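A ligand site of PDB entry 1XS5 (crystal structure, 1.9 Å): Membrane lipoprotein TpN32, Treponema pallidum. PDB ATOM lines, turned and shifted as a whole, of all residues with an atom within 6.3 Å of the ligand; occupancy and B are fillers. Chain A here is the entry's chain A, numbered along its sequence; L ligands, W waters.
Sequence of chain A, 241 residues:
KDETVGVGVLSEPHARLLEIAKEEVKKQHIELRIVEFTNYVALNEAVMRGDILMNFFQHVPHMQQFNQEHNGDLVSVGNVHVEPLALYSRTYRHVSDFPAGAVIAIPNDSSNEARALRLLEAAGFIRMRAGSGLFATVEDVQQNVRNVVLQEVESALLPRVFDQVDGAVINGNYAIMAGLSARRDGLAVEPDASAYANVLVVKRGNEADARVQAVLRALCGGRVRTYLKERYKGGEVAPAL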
ATOM      1  N   LEU A  10     -13.550  -8.048  -3.128  1.00  0.00           N
ATOM      2  CA  LEU A  10     -13.642  -9.025  -4.192  1.00  0.00           C
ATOM      3  C   LEU A  10     -13.206 -10.414  -3.752  1.00  0.00           C
ATOM      4  O   LEU A  10     -13.827 -11.407  -4.120  1.00  0.00           O
ATOM      5  CB  LEU A  10     -12.717  -8.572  -5.345  1.00  0.00           C
ATOM      6  CG  LEU A  10     -12.625  -9.368  -6.647  1.00  0.00           C
ATOM      7  CD1 LEU A  10     -13.960  -9.335  -7.369  1.00  0.00           C
ATOM      8  CD2 LEU A  10     -11.564  -8.690  -7.526  1.00  0.00           C
ATOM      9  N   PRO A  13      -6.528 -11.574  -0.837  1.00  0.00           N
ATOM     10  CA  PRO A  13      -6.282 -11.445   0.609  1.00  0.00           C
ATOM     11  C   PRO A  13      -6.978 -10.263   1.271  1.00  0.00           C
ATOM     12  O   PRO A  13      -6.975 -10.132   2.504  1.00  0.00           O
ATOM     13  CB  PRO A  13      -4.768 -11.284   0.659  1.00  0.00           C
ATOM     14  CG  PRO A  13      -4.530 -10.353  -0.561  1.00  0.00           C
ATOM     15  CD  PRO A  13      -5.373 -11.092  -1.627  1.00  0.00           C
ATOM     16  N   HIS A  14      -7.598  -9.402   0.464  1.00  0.00           N
ATOM     17  CA  HIS A  14      -8.235  -8.209   0.990  1.00  0.00           C
ATOM     18  C   HIS A  14      -9.303  -8.528   2.016  1.00  0.00           C
ATOM     19  O   HIS A  14      -9.495  -7.783   3.000  1.00  0.00           O
ATOM     20  CB  HIS A  14      -8.866  -7.381  -0.158  1.00  0.00           C
ATOM     21  CG  HIS A  14      -7.903  -7.091  -1.279  1.00  0.00           C
ATOM     22  ND1 HIS A  14      -7.254  -8.099  -1.967  1.00  0.00           N
ATOM     23  CD2 HIS A  14      -7.447  -5.925  -1.785  1.00  0.00           C
ATOM     24  CE1 HIS A  14      -6.435  -7.552  -2.861  1.00  0.00           C
ATOM     25  NE2 HIS A  14      -6.530  -6.241  -2.763  1.00  0.00           N
ATOM     26  N   TYR A  40     -15.005  -6.240 -10.988  1.00  0.00           N
ATOM     27  CA  TYR A  40     -14.386  -4.937 -10.815  1.00  0.00           C
ATOM     28  C   TYR A  40     -15.320  -3.703 -10.991  1.00  0.00           C
ATOM     29  O   TYR A  40     -15.313  -2.762 -10.170  1.00  0.00           O
ATOM     30  CB  TYR A  40     -13.193  -4.776 -11.773  1.00  0.00           C
ATOM     31  CG  TYR A  40     -12.043  -5.782 -11.662  1.00  0.00           C
ATOM     32  CD1 TYR A  40     -11.751  -6.453 -10.469  1.00  0.00           C
ATOM     33  CD2 TYR A  40     -11.183  -5.976 -12.757  1.00  0.00           C
ATOM     34  CE1 TYR A  40     -10.608  -7.292 -10.362  1.00  0.00           C
ATOM     35  CE2 TYR A  40     -10.030  -6.828 -12.664  1.00  0.00           C
ATOM     36  CZ  TYR A  40      -9.755  -7.467 -11.466  1.00  0.00           C
ATOM     37  OH  TYR A  40      -8.572  -8.192 -11.377  1.00  0.00           O
ATOM     38  N   PHE A  57      -9.970  -3.258  -3.345  1.00  0.00           N
ATOM     39  CA  PHE A  57      -9.648  -4.359  -4.278  1.00  0.00           C
ATOM     40  C   PHE A  57      -8.743  -3.991  -5.455  1.00  0.00           C
ATOM     41  O   PHE A  57      -8.318  -4.876  -6.171  1.00  0.00           O
ATOM     42  CB  PHE A  57     -10.934  -4.911  -4.913  1.00  0.00           C
ATOM     43  CG  PHE A  57     -11.453  -4.052  -6.052  1.00  0.00           C
ATOM     44  CD1 PHE A  57     -12.136  -2.868  -5.795  1.00  0.00           C
ATOM     45  CD2 PHE A  57     -11.255  -4.441  -7.381  1.00  0.00           C
ATOM     46  CE1 PHE A  57     -12.646  -2.073  -6.850  1.00  0.00           C
ATOM     47  CE2 PHE A  57     -11.742  -3.669  -8.433  1.00  0.00           C
ATOM     48  CZ  PHE A  57     -12.439  -2.486  -8.179  1.00  0.00           C
ATOM     49  N   GLN A  58      -8.429  -2.696  -5.634  1.00  0.00           N
ATOM     50  CA  GLN A  58      -7.712  -2.283  -6.822  1.00  0.00           C
ATOM     51  C   GLN A  58      -6.508  -1.403  -6.547  1.00  0.00           C
ATOM     52  O   GLN A  58      -6.291  -0.987  -5.391  1.00  0.00           O
ATOM     53  CB  GLN A  58      -8.682  -1.483  -7.704  1.00  0.00           C
ATOM     54  CG  GLN A  58      -8.954  -0.028  -7.117  1.00  0.00           C
ATOM     55  CD  GLN A  58     -10.256   0.642  -7.625  1.00  0.00           C
ATOM     56  OE1 GLN A  58     -10.457   0.844  -8.803  1.00  0.00           O
ATOM     57  NE2 GLN A  58     -11.121   0.976  -6.710  1.00  0.00           N
ATOM     58  N   HIS A  59      -5.756  -1.102  -7.616  1.00  0.00           N
ATOM     59  CA  HIS A  59      -4.628  -0.176  -7.496  1.00  0.00           C
ATOM     60  C   HIS A  59      -5.028   1.167  -8.174  1.00  0.00           C
ATOM     61  O   HIS A  59      -6.088   1.256  -8.801  1.00  0.00           O
ATOM     62  CB  HIS A  59      -3.356  -0.796  -8.115  1.00  0.00           C
ATOM     63  CG  HIS A  59      -3.562  -1.465  -9.439  1.00  0.00           C
ATOM     64  ND1 HIS A  59      -4.003  -0.798 -10.559  1.00  0.00           N
ATOM     65  CD2 HIS A  59      -3.311  -2.726  -9.835  1.00  0.00           C
ATOM     66  CE1 HIS A  59      -4.023  -1.623 -11.584  1.00  0.00           C
ATOM     67  NE2 HIS A  59      -3.594  -2.807 -11.165  1.00  0.00           N
ATOM     68  N   HIS A  62      -5.967   1.294 -12.037  1.00  0.00           N
ATOM     69  CA  HIS A  62      -7.278   0.700 -12.308  1.00  0.00           C
ATOM     70  C   HIS A  62      -8.403   1.701 -11.984  1.00  0.00           C
ATOM     71  O   HIS A  62      -9.327   1.854 -12.743  1.00  0.00           O
ATOM     72  CB  HIS A  62      -7.448  -0.595 -11.507  1.00  0.00           C
ATOM     73  CG  HIS A  62      -8.746  -1.292 -11.787  1.00  0.00           C
ATOM     74  ND1 HIS A  62      -9.904  -0.995 -11.111  1.00  0.00           N
ATOM     75  CD2 HIS A  62      -9.071  -2.204 -12.725  1.00  0.00           C
ATOM     76  CE1 HIS A  62     -10.890  -1.712 -11.609  1.00  0.00           C
ATOM     77  NE2 HIS A  62     -10.417  -2.443 -12.600  1.00  0.00           N
ATOM     78  N   HIS A  81      -1.154  -2.219   0.467  1.00  0.00           N
ATOM     79  CA  HIS A  81      -0.236  -3.318   0.242  1.00  0.00           C
ATOM     80  C   HIS A  81       0.111  -3.455  -1.228  1.00  0.00           C
ATOM     81  O   HIS A  81      -0.530  -2.824  -2.054  1.00  0.00           O
ATOM     82  CB  HIS A  81      -0.832  -4.625   0.768  1.00  0.00           C
ATOM     83  CG  HIS A  81      -1.941  -5.206  -0.095  1.00  0.00           C
ATOM     84  ND1 HIS A  81      -3.270  -5.035   0.192  1.00  0.00           N
ATOM     85  CD2 HIS A  81      -1.886  -6.019  -1.178  1.00  0.00           C
ATOM     86  CE1 HIS A  81      -4.004  -5.716  -0.690  1.00  0.00           C
ATOM     87  NE2 HIS A  81      -3.183  -6.325  -1.532  1.00  0.00           N
ATOM     88  N   VAL A  82       1.135  -4.270  -1.517  1.00  0.00           N
ATOM     89  CA  VAL A  82       1.586  -4.552  -2.886  1.00  0.00           C
ATOM     90  C   VAL A  82       1.447  -6.056  -3.113  1.00  0.00           C
ATOM     91  O   VAL A  82       1.698  -6.832  -2.193  1.00  0.00           O
ATOM     92  CB  VAL A  82       3.082  -4.117  -3.140  1.00  0.00           C
ATOM     93  CG1 VAL A  82       3.235  -2.591  -2.952  1.00  0.00           C
ATOM     94  CG2 VAL A  82       4.034  -4.871  -2.203  1.00  0.00           C
ATOM     95  N   GLU A  83       0.997  -6.473  -4.303  1.00  0.00           N
ATOM     96  CA  GLU A  83       0.815  -7.898  -4.638  1.00  0.00           C
ATOM     97  C   GLU A  83       1.582  -8.045  -5.958  1.00  0.00           C
ATOM     98  O   GLU A  83       1.019  -7.734  -7.020  1.00  0.00           O
ATOM     99  CB  GLU A  83      -0.649  -8.135  -4.998  1.00  0.00           C
ATOM    100  CG  GLU A  83      -1.532  -8.783  -4.075  1.00  0.00           C
ATOM    101  CD  GLU A  83      -2.990  -8.633  -4.574  1.00  0.00           C
ATOM    102  OE1 GLU A  83      -3.313  -9.038  -5.710  1.00  0.00           O
ATOM    103  OE2 GLU A  83      -3.783  -8.070  -3.805  1.00  0.00           O
ATOM    104  N   LEU A  85       2.906  -8.957  -9.447  1.00  0.00           N
ATOM    105  CA  LEU A  85       2.354  -9.671 -10.622  1.00  0.00           C
ATOM    106  C   LEU A  85       3.487 -10.565 -11.154  1.00  0.00           C
ATOM    107  O   LEU A  85       4.651 -10.114 -11.237  1.00  0.00           O
ATOM    108  CB  LEU A  85       1.988  -8.664 -11.693  1.00  0.00           C
ATOM    109  CG  LEU A  85       1.357  -9.229 -12.955  1.00  0.00           C
ATOM    110  CD1 LEU A  85      -0.032  -9.750 -12.589  1.00  0.00           C
ATOM    111  CD2 LEU A  85       1.238  -8.134 -13.982  1.00  0.00           C
ATOM    112  N   ASP A 109      -8.348  -6.467 -18.658  1.00  0.00           N
ATOM    113  CA  ASP A 109      -8.798  -5.112 -18.307  1.00  0.00           C
ATOM    114  C   ASP A 109      -7.544  -4.266 -18.558  1.00  0.00           C
ATOM    115  O   ASP A 109      -6.430  -4.601 -18.138  1.00  0.00           O
ATOM    116  CB  ASP A 109      -9.295  -5.003 -16.875  1.00  0.00           C
ATOM    117  CG  ASP A 109      -8.248  -5.371 -15.850  1.00  0.00           C
ATOM    118  OD1 ASP A 109      -7.892  -6.561 -15.749  1.00  0.00           O
ATOM    119  OD2 ASP A 109      -7.792  -4.465 -15.126  1.00  0.00           O
ATOM    120  N   SER A 111      -5.719  -1.549 -17.573  1.00  0.00           N
ATOM    121  CA  SER A 111      -4.575  -1.212 -16.723  1.00  0.00           C
ATOM    122  C   SER A 111      -3.730  -2.450 -16.321  1.00  0.00           C
ATOM    123  O   SER A 111      -2.511  -2.341 -16.174  1.00  0.00           O
ATOM    124  CB  SER A 111      -5.030  -0.442 -15.469  1.00  0.00           C
ATOM    125  OG  SER A 111      -5.782  -1.252 -14.597  1.00  0.00           O
ATOM    126  N   ASN A 112      -4.362  -3.616 -16.124  1.00  0.00           N
ATOM    127  CA  ASN A 112      -3.582  -4.800 -15.779  1.00  0.00           C
ATOM    128  C   ASN A 112      -3.030  -5.487 -16.993  1.00  0.00           C
ATOM    129  O   ASN A 112      -2.056  -6.225 -16.894  1.00  0.00           O
ATOM    130  CB  ASN A 112      -4.418  -5.757 -14.917  1.00  0.00           C
ATOM    131  CG  ASN A 112      -4.633  -5.182 -13.547  1.00  0.00           C
ATOM    132  OD1 ASN A 112      -3.657  -5.040 -12.791  1.00  0.00           O
ATOM    133  ND2 ASN A 112      -5.873  -4.748 -13.230  1.00  0.00           N
ATOM    134  N   ARG A 115       0.148  -3.589 -17.573  1.00  0.00           N
ATOM    135  CA  ARG A 115       1.072  -4.013 -16.526  1.00  0.00           C
ATOM    136  C   ARG A 115       1.706  -5.367 -16.865  1.00  0.00           C
ATOM    137  O   ARG A 115       2.928  -5.561 -16.691  1.00  0.00           O
ATOM    138  CB  ARG A 115       0.274  -4.099 -15.215  1.00  0.00           C
ATOM    139  CG  ARG A 115       1.069  -4.439 -13.986  1.00  0.00           C
ATOM    140  CD  ARG A 115       0.073  -4.575 -12.846  1.00  0.00           C
ATOM    141  NE  ARG A 115       0.738  -4.965 -11.599  1.00  0.00           N
ATOM    142  CZ  ARG A 115       0.052  -5.369 -10.552  1.00  0.00           C
ATOM    143  NH1 ARG A 115      -1.261  -5.433 -10.670  1.00  0.00           N
ATOM    144  NH2 ARG A 115       0.648  -5.663  -9.391  1.00  0.00           N
ATOM    145  N   ASN A 171      -2.718 -11.990 -11.640  1.00  0.00           N
ATOM    146  CA  ASN A 171      -2.719 -11.071 -10.482  1.00  0.00           C
ATOM    147  C   ASN A 171      -2.473 -11.876  -9.188  1.00  0.00           C
ATOM    148  O   ASN A 171      -3.031 -12.981  -9.024  1.00  0.00           O
ATOM    149  CB  ASN A 171      -4.063 -10.389 -10.255  1.00  0.00           C
ATOM    150  CG  ASN A 171      -4.534  -9.612 -11.482  1.00  0.00           C
ATOM    151  OD1 ASN A 171      -4.991 -10.221 -12.450  1.00  0.00           O
ATOM    152  ND2 ASN A 171      -4.394  -8.295 -11.451  1.00  0.00           N
ATOM    153  N   GLY A 172      -1.774 -11.263  -8.251  1.00  0.00           N
ATOM    154  CA  GLY A 172      -1.476 -11.958  -7.003  1.00  0.00           C
ATOM    155  C   GLY A 172      -2.696 -12.503  -6.276  1.00  0.00           C
ATOM    156  O   GLY A 172      -2.662 -13.650  -5.827  1.00  0.00           O
ATOM    157  N   ASN A 173      -3.777 -11.728  -6.180  1.00  0.00           N
ATOM    158  CA  ASN A 173      -4.915 -12.269  -5.439  1.00  0.00           C
ATOM    159  C   ASN A 173      -5.423 -13.574  -6.040  1.00  0.00           C
ATOM    160  O   ASN A 173      -5.655 -14.593  -5.332  1.00  0.00           O
ATOM    161  CB  ASN A 173      -6.067 -11.215  -5.339  1.00  0.00           C
ATOM    162  CG  ASN A 173      -6.719 -10.916  -6.678  1.00  0.00           C
ATOM    163  OD1 ASN A 173      -6.087 -10.401  -7.605  1.00  0.00           O
ATOM    164  ND2 ASN A 173      -8.008 -11.248  -6.778  1.00  0.00           N
ATOM    165  N   TYR A 196       1.764  -0.290  -8.325  1.00  0.00           N
ATOM    166  CA  TYR A 196       0.458  -0.927  -8.368  1.00  0.00           C
ATOM    167  C   TYR A 196      -0.039  -1.326  -7.001  1.00  0.00           C
ATOM    168  O   TYR A 196      -0.794  -2.289  -6.857  1.00  0.00           O
ATOM    169  CB  TYR A 196       0.555  -2.109  -9.344  1.00  0.00           C
ATOM    170  CG  TYR A 196       0.702  -1.625 -10.781  1.00  0.00           C
ATOM    171  CD1 TYR A 196      -0.433  -1.221 -11.519  1.00  0.00           C
ATOM    172  CD2 TYR A 196       1.953  -1.523 -11.395  1.00  0.00           C
ATOM    173  CE1 TYR A 196      -0.308  -0.756 -12.821  1.00  0.00           C
ATOM    174  CE2 TYR A 196       2.084  -1.039 -12.703  1.00  0.00           C
ATOM    175  CZ  TYR A 196       0.939  -0.661 -13.412  1.00  0.00           C
ATOM    176  OH  TYR A 196       1.043  -0.220 -14.718  1.00  0.00           O
ATOM    177  N   ALA A 197       0.373  -0.559  -5.986  1.00  0.00           N
ATOM    178  CA  ALA A 197      -0.094  -0.782  -4.598  1.00  0.00           C
ATOM    179  C   ALA A 197      -1.630  -0.690  -4.592  1.00  0.00           C
ATOM    180  O   ALA A 197      -2.241   0.157  -5.281  1.00  0.00           O
ATOM    181  CB  ALA A 197       0.496   0.308  -3.661  1.00  0.00           C
ATOM    182  N   ASN A 198      -2.253  -1.580  -3.815  1.00  0.00           N
ATOM    183  CA  ASN A 198      -3.710  -1.646  -3.684  1.00  0.00           C
ATOM    184  C   ASN A 198      -4.102  -0.613  -2.660  1.00  0.00           C
ATOM    185  O   ASN A 198      -3.465  -0.477  -1.604  1.00  0.00           O
ATOM    186  CB  ASN A 198      -4.125  -3.045  -3.261  1.00  0.00           C
ATOM    187  CG  ASN A 198      -4.110  -4.041  -4.440  1.00  0.00           C
ATOM    188  OD1 ASN A 198      -4.968  -4.930  -4.512  1.00  0.00           O
ATOM    189  ND2 ASN A 198      -3.139  -3.891  -5.359  1.00  0.00           N
HETATM  190  N1  LIG L   1      -5.191  -7.226  -6.319  1.00  0.00           N
HETATM  191  C1  LIG L   1      -4.981  -6.836  -7.760  1.00  0.00           C
HETATM  192  C2  LIG L   1      -3.506  -6.609  -8.130  1.00  0.00           C
HETATM  193  O1  LIG L   1      -3.055  -7.127  -9.180  1.00  0.00           O
HETATM  194  C3  LIG L   1      -5.763  -5.544  -8.084  1.00  0.00           C
HETATM  195  C4  LIG L   1      -5.834  -5.281  -9.570  1.00  0.00           C
HETATM  196  S1  LIG L   1      -6.699  -3.755 -10.018  1.00  0.00           S
HETATM  197  C5  LIG L   1      -8.429  -4.361  -9.859  1.00  0.00           C
HETATM  198  O2  LIG L   1      -2.810  -5.912  -7.361  1.00  0.00           O
HETATM  199  O   HOH W   1      -0.780  -8.838  -8.900  1.00  0.00           O
HETATM  200  O   HOH W   2      -0.410  -4.824  -6.381  1.00  0.00           O
HETATM  201  O   HOH W   3      -7.953  -7.538  -6.173  1.00  0.00           O
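Water W3 lies within hydrogen-bond range of O of Phe 57 (2.7 Å) and N1 of the ligand (2.8 Å). Water W1 lies within hydrogen-bond range of N of Gly 172 (2.7 Å), O of Glu 83 (2.8 Å) and O1 of the ligand (2.9 Å).
Merely in contact with the ligand: His 14 (3.7 Å), Tyr 40 (3.7 Å), Phe 57 (3.3 Å), Gln 58 (3.6 Å), His 62 (3.6 Å) and Asn 173 (3.5 Å). Hydrophobic or aromatic side chains within 4 Å of the ligand: His 14, Tyr 40, Phe 57, His 59 and His 62. Of the 22 residues printed, 12 come within 4 Å of the ligand. The nearest printed residue that does not touch the ligand is Tyr 196 (4.2 Å).
OE1 of Glu 83 sits at hydrogen-bond distance from N of Asn 173, at 2.8 Å. OE2 of Glu 83 sits at hydrogen-bond distance from NE2 of His 81, at 2.9 Å. OD1 of Asn 198 is in hydrogen-bond range of NE2 of His 14, 2.7 Å away. The side-chain amide oxygen of Asn 112 sits at hydrogen-bond distance from a ring nitrogen (NE2) of His 59 (2.8 Å). The backbone carbonyl oxygen (O) of Glu 83 sits at hydrogen-bond distance from the guanidinium group (NH2) of Arg 115, at 3.2 Å. A ring nitrogen (ND1) of His 62 is in hydrogen-bond range of the side-chain amide oxygen of Gln 58 (3.0 Å). The side-chain carboxylate (OE2) of Glu 83 lies close to the side-chain amide oxygen (OD1) of Asn 198 (3.4 Å). A ring nitrogen (ND1) of His 59 is in hydrogen-bond range of the backbone NH (N) of His 62, at 3.2 Å.
S1 of the ligand sits close to ND2 of Asn 112 (3.5 Å). A sulfur (S1) of the ligand lies close to a ring nitrogen (NE2) of His 59, at 3.4 Å. ND2 of Asn 198 lies within hydrogen-bond range of O2 of the ligand (2.9 Å). A nitrogen (N1) of the ligand is in salt-bridge range of the side-chain carboxylate (OE1) of Glu 83, at 2.7 Å. ND2 of Asn 171 is in hydrogen-bond range of O1 of the ligand, 2.9 Å away. The guanidinium group (NH1) of Arg 115 is in salt-bridge range of an oxygen (O1) of the ligand (2.9 Å). S1 of the ligand lies close to N of His 59, at 3.7 Å.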
